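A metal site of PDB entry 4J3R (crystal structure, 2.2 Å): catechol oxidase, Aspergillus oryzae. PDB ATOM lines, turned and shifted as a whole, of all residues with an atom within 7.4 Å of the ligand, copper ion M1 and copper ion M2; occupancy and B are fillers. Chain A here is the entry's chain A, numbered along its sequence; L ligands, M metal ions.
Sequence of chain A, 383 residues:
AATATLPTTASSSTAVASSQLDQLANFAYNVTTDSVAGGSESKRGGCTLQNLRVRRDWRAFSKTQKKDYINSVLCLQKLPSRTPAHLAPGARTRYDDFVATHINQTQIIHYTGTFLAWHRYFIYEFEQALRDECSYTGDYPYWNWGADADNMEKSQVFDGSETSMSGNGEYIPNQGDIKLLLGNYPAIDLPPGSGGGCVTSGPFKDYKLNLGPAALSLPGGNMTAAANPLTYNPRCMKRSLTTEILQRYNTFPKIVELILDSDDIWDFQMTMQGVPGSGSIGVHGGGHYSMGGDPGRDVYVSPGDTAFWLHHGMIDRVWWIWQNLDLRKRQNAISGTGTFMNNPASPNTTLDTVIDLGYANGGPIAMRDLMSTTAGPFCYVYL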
ATOM      1  N   HIS A 102       8.137  23.719   7.349  1.00  0.00           N
ATOM      2  CA  HIS A 102       7.741  22.514   8.069  1.00  0.00           C
ATOM      3  C   HIS A 102       8.344  21.270   7.424  1.00  0.00           C
ATOM      4  O   HIS A 102       8.825  20.359   8.113  1.00  0.00           O
ATOM      5  CB  HIS A 102       6.223  22.392   8.130  1.00  0.00           C
ATOM      6  CG  HIS A 102       5.755  21.342   9.082  1.00  0.00           C
ATOM      7  ND1 HIS A 102       5.550  20.026   8.707  1.00  0.00           N
ATOM      8  CD2 HIS A 102       5.471  21.401  10.401  1.00  0.00           C
ATOM      9  CE1 HIS A 102       5.135  19.328   9.742  1.00  0.00           C
ATOM     10  NE2 HIS A 102       5.087  20.140  10.785  1.00  0.00           N
ATOM     11  N   GLN A 105      12.097  20.997   8.119  1.00  0.00           N
ATOM     12  CA  GLN A 105      12.522  20.755   9.495  1.00  0.00           C
ATOM     13  C   GLN A 105      11.811  19.576  10.174  1.00  0.00           C
ATOM     14  O   GLN A 105      11.930  19.414  11.392  1.00  0.00           O
ATOM     15  CB  GLN A 105      12.312  22.001  10.351  1.00  0.00           C
ATOM     16  CG  GLN A 105      13.014  23.261   9.851  1.00  0.00           C
ATOM     17  CD  GLN A 105      13.024  24.376  10.913  1.00  0.00           C
ATOM     18  OE1 GLN A 105      13.403  24.143  12.063  1.00  0.00           O
ATOM     19  NE2 GLN A 105      12.600  25.569  10.533  1.00  0.00           N
ATOM     20  N   THR A 106      11.091  18.770   9.400  1.00  0.00           N
ATOM     21  CA  THR A 106      10.258  17.706   9.959  1.00  0.00           C
ATOM     22  C   THR A 106      11.021  16.735  10.856  1.00  0.00           C
ATOM     23  O   THR A 106      10.517  16.303  11.880  1.00  0.00           O
ATOM     24  CB  THR A 106       9.519  16.927   8.829  1.00  0.00           C
ATOM     25  OG1 THR A 106       8.366  17.671   8.426  1.00  0.00           O
ATOM     26  CG2 THR A 106       9.083  15.556   9.289  1.00  0.00           C
ATOM     27  N   ILE A 109      11.591  18.335  14.477  1.00  0.00           N
ATOM     28  CA  ILE A 109      10.499  18.995  15.205  1.00  0.00           C
ATOM     29  C   ILE A 109       9.380  18.050  15.637  1.00  0.00           C
ATOM     30  O   ILE A 109       8.387  18.479  16.198  1.00  0.00           O
ATOM     31  CB  ILE A 109       9.884  20.155  14.399  1.00  0.00           C
ATOM     32  CG1 ILE A 109       9.228  19.622  13.114  1.00  0.00           C
ATOM     33  CG2 ILE A 109      10.931  21.235  14.113  1.00  0.00           C
ATOM     34  CD1 ILE A 109       8.585  20.720  12.282  1.00  0.00           C
ATOM     35  N   HIS A 110       9.547  16.753  15.376  1.00  0.00           N
ATOM     36  CA  HIS A 110       8.591  15.764  15.832  1.00  0.00           C
ATOM     37  C   HIS A 110       9.350  14.733  16.637  1.00  0.00           C
ATOM     38  O   HIS A 110      10.480  14.393  16.293  1.00  0.00           O
ATOM     39  CB  HIS A 110       7.843  15.124  14.651  1.00  0.00           C
ATOM     40  CG  HIS A 110       7.051  16.099  13.842  1.00  0.00           C
ATOM     41  ND1 HIS A 110       7.499  16.623  12.645  1.00  0.00           N
ATOM     42  CD2 HIS A 110       5.833  16.649  14.054  1.00  0.00           C
ATOM     43  CE1 HIS A 110       6.594  17.452  12.159  1.00  0.00           C
ATOM     44  NE2 HIS A 110       5.573  17.490  12.989  1.00  0.00           N
ATOM     45  N   PHE A 115       9.349  19.750  19.938  1.00  0.00           N
ATOM     46  CA  PHE A 115       8.057  19.535  19.250  1.00  0.00           C
ATOM     47  C   PHE A 115       6.918  20.490  19.665  1.00  0.00           C
ATOM     48  O   PHE A 115       6.362  21.206  18.818  1.00  0.00           O
ATOM     49  CB  PHE A 115       7.607  18.081  19.410  1.00  0.00           C
ATOM     50  CG  PHE A 115       6.170  17.850  19.054  1.00  0.00           C
ATOM     51  CD1 PHE A 115       5.749  17.884  17.730  1.00  0.00           C
ATOM     52  CD2 PHE A 115       5.240  17.579  20.038  1.00  0.00           C
ATOM     53  CE1 PHE A 115       4.416  17.676  17.406  1.00  0.00           C
ATOM     54  CE2 PHE A 115       3.907  17.365  19.730  1.00  0.00           C
ATOM     55  CZ  PHE A 115       3.495  17.410  18.410  1.00  0.00           C
ATOM     56  N   TRP A 118       8.026  24.383  19.301  1.00  0.00           N
ATOM     57  CA  TRP A 118       8.184  24.753  17.904  1.00  0.00           C
ATOM     58  C   TRP A 118       6.819  24.978  17.250  1.00  0.00           C
ATOM     59  O   TRP A 118       6.596  26.000  16.583  1.00  0.00           O
ATOM     60  CB  TRP A 118       8.991  23.701  17.141  1.00  0.00           C
ATOM     61  CG  TRP A 118       9.360  24.110  15.764  1.00  0.00           C
ATOM     62  CD1 TRP A 118      10.564  24.626  15.351  1.00  0.00           C
ATOM     63  CD2 TRP A 118       8.532  24.037  14.598  1.00  0.00           C
ATOM     64  NE1 TRP A 118      10.526  24.866  14.001  1.00  0.00           N
ATOM     65  CE2 TRP A 118       9.291  24.525  13.512  1.00  0.00           C
ATOM     66  CE3 TRP A 118       7.212  23.610  14.371  1.00  0.00           C
ATOM     67  CZ2 TRP A 118       8.775  24.595  12.212  1.00  0.00           C
ATOM     68  CZ3 TRP A 118       6.703  23.674  13.075  1.00  0.00           C
ATOM     69  CH2 TRP A 118       7.493  24.161  12.011  1.00  0.00           C
ATOM     70  N   HIS A 119       5.897  24.055  17.453  1.00  0.00           N
ATOM     71  CA  HIS A 119       4.580  24.208  16.833  1.00  0.00           C
ATOM     72  C   HIS A 119       3.827  25.380  17.450  1.00  0.00           C
ATOM     73  O   HIS A 119       3.083  26.089  16.757  1.00  0.00           O
ATOM     74  CB  HIS A 119       3.784  22.897  16.907  1.00  0.00           C
ATOM     75  CG  HIS A 119       4.300  21.849  15.966  1.00  0.00           C
ATOM     76  ND1 HIS A 119       5.421  21.092  16.245  1.00  0.00           N
ATOM     77  CD2 HIS A 119       3.872  21.452  14.750  1.00  0.00           C
ATOM     78  CE1 HIS A 119       5.648  20.264  15.240  1.00  0.00           C
ATOM     79  NE2 HIS A 119       4.723  20.470  14.318  1.00  0.00           N
ATOM     80  N   PHE A 122       5.302  28.156  15.576  1.00  0.00           N
ATOM     81  CA  PHE A 122       4.865  28.045  14.176  1.00  0.00           C
ATOM     82  C   PHE A 122       3.495  28.716  13.979  1.00  0.00           C
ATOM     83  O   PHE A 122       3.347  29.643  13.173  1.00  0.00           O
ATOM     84  CB  PHE A 122       4.816  26.562  13.768  1.00  0.00           C
ATOM     85  CG  PHE A 122       4.727  26.321  12.280  1.00  0.00           C
ATOM     86  CD1 PHE A 122       5.503  27.039  11.385  1.00  0.00           C
ATOM     87  CD2 PHE A 122       3.901  25.321  11.789  1.00  0.00           C
ATOM     88  CE1 PHE A 122       5.420  26.789  10.004  1.00  0.00           C
ATOM     89  CE2 PHE A 122       3.819  25.060  10.416  1.00  0.00           C
ATOM     90  CZ  PHE A 122       4.576  25.797   9.534  1.00  0.00           C
ATOM     91  N   GLN A 273       1.680  12.190  20.914  1.00  0.00           N
ATOM     92  CA  GLN A 273       2.129  11.876  19.562  1.00  0.00           C
ATOM     93  C   GLN A 273       1.915  10.411  19.200  1.00  0.00           C
ATOM     94  O   GLN A 273       1.934  10.055  18.022  1.00  0.00           O
ATOM     95  CB  GLN A 273       3.611  12.230  19.384  1.00  0.00           C
ATOM     96  CG  GLN A 273       3.844  13.702  19.151  1.00  0.00           C
ATOM     97  CD  GLN A 273       5.304  14.083  19.306  1.00  0.00           C
ATOM     98  OE1 GLN A 273       6.016  14.270  18.324  1.00  0.00           O
ATOM     99  NE2 GLN A 273       5.745  14.207  20.559  1.00  0.00           N
ATOM    100  N   HIS A 284      -2.610  13.636  18.493  1.00  0.00           N
ATOM    101  CA  HIS A 284      -1.922  14.379  17.452  1.00  0.00           C
ATOM    102  C   HIS A 284      -1.998  13.644  16.117  1.00  0.00           C
ATOM    103  O   HIS A 284      -2.291  14.251  15.104  1.00  0.00           O
ATOM    104  CB  HIS A 284      -0.461  14.649  17.802  1.00  0.00           C
ATOM    105  CG  HIS A 284       0.284  15.347  16.713  1.00  0.00           C
ATOM    106  ND1 HIS A 284       1.304  14.751  16.009  1.00  0.00           N
ATOM    107  CD2 HIS A 284       0.137  16.588  16.187  1.00  0.00           C
ATOM    108  CE1 HIS A 284       1.761  15.589  15.104  1.00  0.00           C
ATOM    109  NE2 HIS A 284       1.062  16.708  15.177  1.00  0.00           N
ATOM    110  N   GLY A 285      -1.731  12.336  16.139  1.00  0.00           N
ATOM    111  CA  GLY A 285      -1.803  11.511  14.946  1.00  0.00           C
ATOM    112  C   GLY A 285      -3.229  11.368  14.472  1.00  0.00           C
ATOM    113  O   GLY A 285      -3.517  11.519  13.283  1.00  0.00           O
ATOM    114  N   HIS A 288      -4.473  14.449  12.660  1.00  0.00           N
ATOM    115  CA  HIS A 288      -3.884  14.497  11.322  1.00  0.00           C
ATOM    116  C   HIS A 288      -4.511  13.484  10.376  1.00  0.00           C
ATOM    117  O   HIS A 288      -5.030  13.845   9.325  1.00  0.00           O
ATOM    118  CB  HIS A 288      -2.379  14.276  11.391  1.00  0.00           C
ATOM    119  CG  HIS A 288      -1.613  15.502  11.748  1.00  0.00           C
ATOM    120  ND1 HIS A 288      -1.590  16.632  10.957  1.00  0.00           N
ATOM    121  CD2 HIS A 288      -0.834  15.790  12.823  1.00  0.00           C
ATOM    122  CE1 HIS A 288      -0.829  17.550  11.516  1.00  0.00           C
ATOM    123  NE2 HIS A 288      -0.362  17.062  12.645  1.00  0.00           N
ATOM    124  N   ASP A 298       0.723  12.968   5.102  1.00  0.00           N
ATOM    125  CA  ASP A 298       2.138  13.198   4.899  1.00  0.00           C
ATOM    126  C   ASP A 298       2.677  13.986   6.097  1.00  0.00           C
ATOM    127  O   ASP A 298       2.400  15.183   6.234  1.00  0.00           O
ATOM    128  CB  ASP A 298       2.324  13.963   3.594  1.00  0.00           C
ATOM    129  CG  ASP A 298       3.785  14.080   3.169  1.00  0.00           C
ATOM    130  OD1 ASP A 298       4.635  14.427   4.016  1.00  0.00           O
ATOM    131  OD2 ASP A 298       4.074  13.856   1.971  1.00  0.00           O
ATOM    132  N   VAL A 299       3.438  13.333   6.960  1.00  0.00           N
ATOM    133  CA  VAL A 299       3.961  13.988   8.158  1.00  0.00           C
ATOM    134  C   VAL A 299       4.688  15.303   7.840  1.00  0.00           C
ATOM    135  O   VAL A 299       4.569  16.268   8.567  1.00  0.00           O
ATOM    136  CB  VAL A 299       4.878  13.063   8.977  1.00  0.00           C
ATOM    137  CG1 VAL A 299       5.407  13.811  10.181  1.00  0.00           C
ATOM    138  CG2 VAL A 299       4.098  11.842   9.445  1.00  0.00           C
ATOM    139  N   TYR A 300       5.400  15.360   6.718  1.00  0.00           N
ATOM    140  CA  TYR A 300       6.177  16.567   6.398  1.00  0.00           C
ATOM    141  C   TYR A 300       5.313  17.706   5.890  1.00  0.00           C
ATOM    142  O   TYR A 300       5.592  18.858   6.176  1.00  0.00           O
ATOM    143  CB  TYR A 300       7.187  16.274   5.296  1.00  0.00           C
ATOM    144  CG  TYR A 300       8.242  15.251   5.606  1.00  0.00           C
ATOM    145  CD1 TYR A 300       9.581  15.620   5.672  1.00  0.00           C
ATOM    146  CD2 TYR A 300       7.917  13.912   5.802  1.00  0.00           C
ATOM    147  CE1 TYR A 300      10.568  14.687   5.937  1.00  0.00           C
ATOM    148  CE2 TYR A 300       8.890  12.968   6.076  1.00  0.00           C
ATOM    149  CZ  TYR A 300      10.216  13.362   6.152  1.00  0.00           C
ATOM    150  OH  TYR A 300      11.189  12.435   6.401  1.00  0.00           O
ATOM    151  N   VAL A 301       4.297  17.372   5.105  1.00  0.00           N
ATOM    152  CA  VAL A 301       3.616  18.350   4.254  1.00  0.00           C
ATOM    153  C   VAL A 301       2.269  18.745   4.860  1.00  0.00           C
ATOM    154  O   VAL A 301       1.579  19.624   4.348  1.00  0.00           O
ATOM    155  CB  VAL A 301       3.449  17.768   2.804  1.00  0.00           C
ATOM    156  CG1 VAL A 301       2.983  18.827   1.816  1.00  0.00           C
ATOM    157  CG2 VAL A 301       4.761  17.211   2.347  1.00  0.00           C
ATOM    158  N   SER A 302       1.929  18.120   5.982  1.00  0.00           N
ATOM    159  CA  SER A 302       0.655  18.362   6.655  1.00  0.00           C
ATOM    160  C   SER A 302       0.170  19.822   6.811  1.00  0.00           C
ATOM    161  O   SER A 302      -1.039  20.047   6.788  1.00  0.00           O
ATOM    162  CB  SER A 302       0.611  17.641   8.009  1.00  0.00           C
ATOM    163  OG  SER A 302       1.525  18.234   8.903  1.00  0.00           O
ATOM    164  N   PRO A 303       1.080  20.801   6.944  1.00  0.00           N
ATOM    165  CA  PRO A 303       0.511  22.155   7.027  1.00  0.00           C
ATOM    166  C   PRO A 303      -0.104  22.643   5.718  1.00  0.00           C
ATOM    167  O   PRO A 303      -0.715  23.707   5.695  1.00  0.00           O
ATOM    168  CB  PRO A 303       1.723  23.038   7.380  1.00  0.00           C
ATOM    169  CG  PRO A 303       2.706  22.096   7.964  1.00  0.00           C
ATOM    170  CD  PRO A 303       2.525  20.810   7.239  1.00  0.00           C
ATOM    171  N   PHE A 308      -4.702  22.153   9.378  1.00  0.00           N
ATOM    172  CA  PHE A 308      -3.507  22.037  10.211  1.00  0.00           C
ATOM    173  C   PHE A 308      -3.504  23.062  11.353  1.00  0.00           C
ATOM    174  O   PHE A 308      -3.241  22.709  12.495  1.00  0.00           O
ATOM    175  CB  PHE A 308      -2.253  22.221   9.362  1.00  0.00           C
ATOM    176  CG  PHE A 308      -0.973  22.167  10.139  1.00  0.00           C
ATOM    177  CD1 PHE A 308      -0.508  23.305  10.812  1.00  0.00           C
ATOM    178  CD2 PHE A 308      -0.225  21.001  10.193  1.00  0.00           C
ATOM    179  CE1 PHE A 308       0.676  23.273  11.534  1.00  0.00           C
ATOM    180  CE2 PHE A 308       0.967  20.963  10.919  1.00  0.00           C
ATOM    181  CZ  PHE A 308       1.417  22.096  11.585  1.00  0.00           C
ATOM    182  N   HIS A 311      -6.066  22.331  14.066  1.00  0.00           N
ATOM    183  CA  HIS A 311      -5.611  21.127  14.775  1.00  0.00           C
ATOM    184  C   HIS A 311      -4.537  21.487  15.822  1.00  0.00           C
ATOM    185  O   HIS A 311      -4.623  21.095  16.987  1.00  0.00           O
ATOM    186  CB  HIS A 311      -5.054  20.120  13.773  1.00  0.00           C
ATOM    187  CG  HIS A 311      -4.487  18.877  14.397  1.00  0.00           C
ATOM    188  ND1 HIS A 311      -5.161  18.142  15.342  1.00  0.00           N
ATOM    189  CD2 HIS A 311      -3.310  18.237  14.194  1.00  0.00           C
ATOM    190  CE1 HIS A 311      -4.429  17.107  15.702  1.00  0.00           C
ATOM    191  NE2 HIS A 311      -3.300  17.135  15.022  1.00  0.00           N
ATOM    192  N   HIS A 312      -3.537  22.248  15.391  1.00  0.00           N
ATOM    193  CA  HIS A 312      -2.457  22.587  16.277  1.00  0.00           C
ATOM    194  C   HIS A 312      -2.838  23.685  17.264  1.00  0.00           C
ATOM    195  O   HIS A 312      -2.200  23.831  18.288  1.00  0.00           O
ATOM    196  CB  HIS A 312      -1.172  22.892  15.522  1.00  0.00           C
ATOM    197  CG  HIS A 312      -0.342  21.673  15.305  1.00  0.00           C
ATOM    198  ND1 HIS A 312       0.581  21.225  16.232  1.00  0.00           N
ATOM    199  CD2 HIS A 312      -0.362  20.752  14.314  1.00  0.00           C
ATOM    200  CE1 HIS A 312       1.116  20.095  15.799  1.00  0.00           C
ATOM    201  NE2 HIS A 312       0.571  19.789  14.632  1.00  0.00           N
ATOM    202  N   ILE A 315      -3.873  21.307  19.762  1.00  0.00           N
ATOM    203  CA  ILE A 315      -2.689  20.699  20.361  1.00  0.00           C
ATOM    204  C   ILE A 315      -2.073  21.646  21.407  1.00  0.00           C
ATOM    205  O   ILE A 315      -1.751  21.231  22.524  1.00  0.00           O
ATOM    206  CB  ILE A 315      -1.638  20.329  19.298  1.00  0.00           C
ATOM    207  CG1 ILE A 315      -2.170  19.224  18.372  1.00  0.00           C
ATOM    208  CG2 ILE A 315      -0.331  19.877  19.953  1.00  0.00           C
ATOM    209  CD1 ILE A 315      -2.233  17.862  19.040  1.00  0.00           C
HETATM  210  O1  LIG L   1       2.751  17.900  11.897  1.00  0.00           O
HETATM  211  O2  LIG L   1       3.064  18.329  12.978  1.00  0.00           O
HETATM  212 CU    CU M   1       4.786  19.442  12.556  1.00  0.00          CU
HETATM  213 CU    CU M   2       0.885  18.124  13.749  1.00  0.00          CU
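Copper ion M2 is bound by a ring nitrogen (NE2) of His 312 (1.9 Å), a ring nitrogen (NE2) of His 288 (2.0 Å), a ring nitrogen (NE2) of His 284 (2.0 Å) and an oxygen (O2) of the ligand (2.3 Å).
Three residues have an atom within 4 Å of copper ion M2: His 284, His 288 and His 312. The nearest printed residue that does not touch copper ion M2 is Phe 308 (4.01 Å).
The side-chain hydroxyl (OG) of Ser 302 sits at hydrogen-bond distance from an oxygen (O1) of the ligand (3.3 Å).
Three residues have an atom within 4 Å of copper ion M1: His 102, His 110 and His 119. Along chain A the residues within 4 Å of copper ion M1 span positions 102 to 119. The nearest printed residue that does not touch copper ion M1 is Ile 109 (4.02 Å).
NE2 of His 102 is bound to copper ion M1, at 1.9 Å. NE2 of His 119 is bound to copper ion M1 (2.0 Å). Copper ion M1 is bound by O2 of the ligand (2.1 Å). A ring nitrogen (NE2) of His 110 is bound to copper ion M1.
The backbone carbonyl oxygen (O) of His 102 sits at hydrogen-bond distance from the side-chain hydroxyl (OG1) of Thr 106, at 2.7 Å. A ring nitrogen (ND1) of His 102 lies within hydrogen-bond range of the backbone carbonyl oxygen of Tyr 300 (2.8 Å). The backbone carbonyl oxygen (O) of His 284 lies within hydrogen-bond range of a ring nitrogen (NE2) of His 311, at 3.1 Å. A ring nitrogen (ND1) of His 119 sits at hydrogen-bond distance from the backbone carbonyl oxygen (O) of Phe 115, at 2.7 Å. The backbone carbonyl oxygen of Thr 106 sits at hydrogen-bond distance from a ring nitrogen (ND1) of His 110.
Merely in contact with the ligand: Phe 308. Hydrophobic or aromatic side chains that line the ligand: His 102, His 110, His 119, His 284, His 288, Phe 308 and His 312. Of the 23 residues printed, 8 come within 4 Å of the ligand. Along chain A the residues within 4 Å of the ligand span positions 102 to 312.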
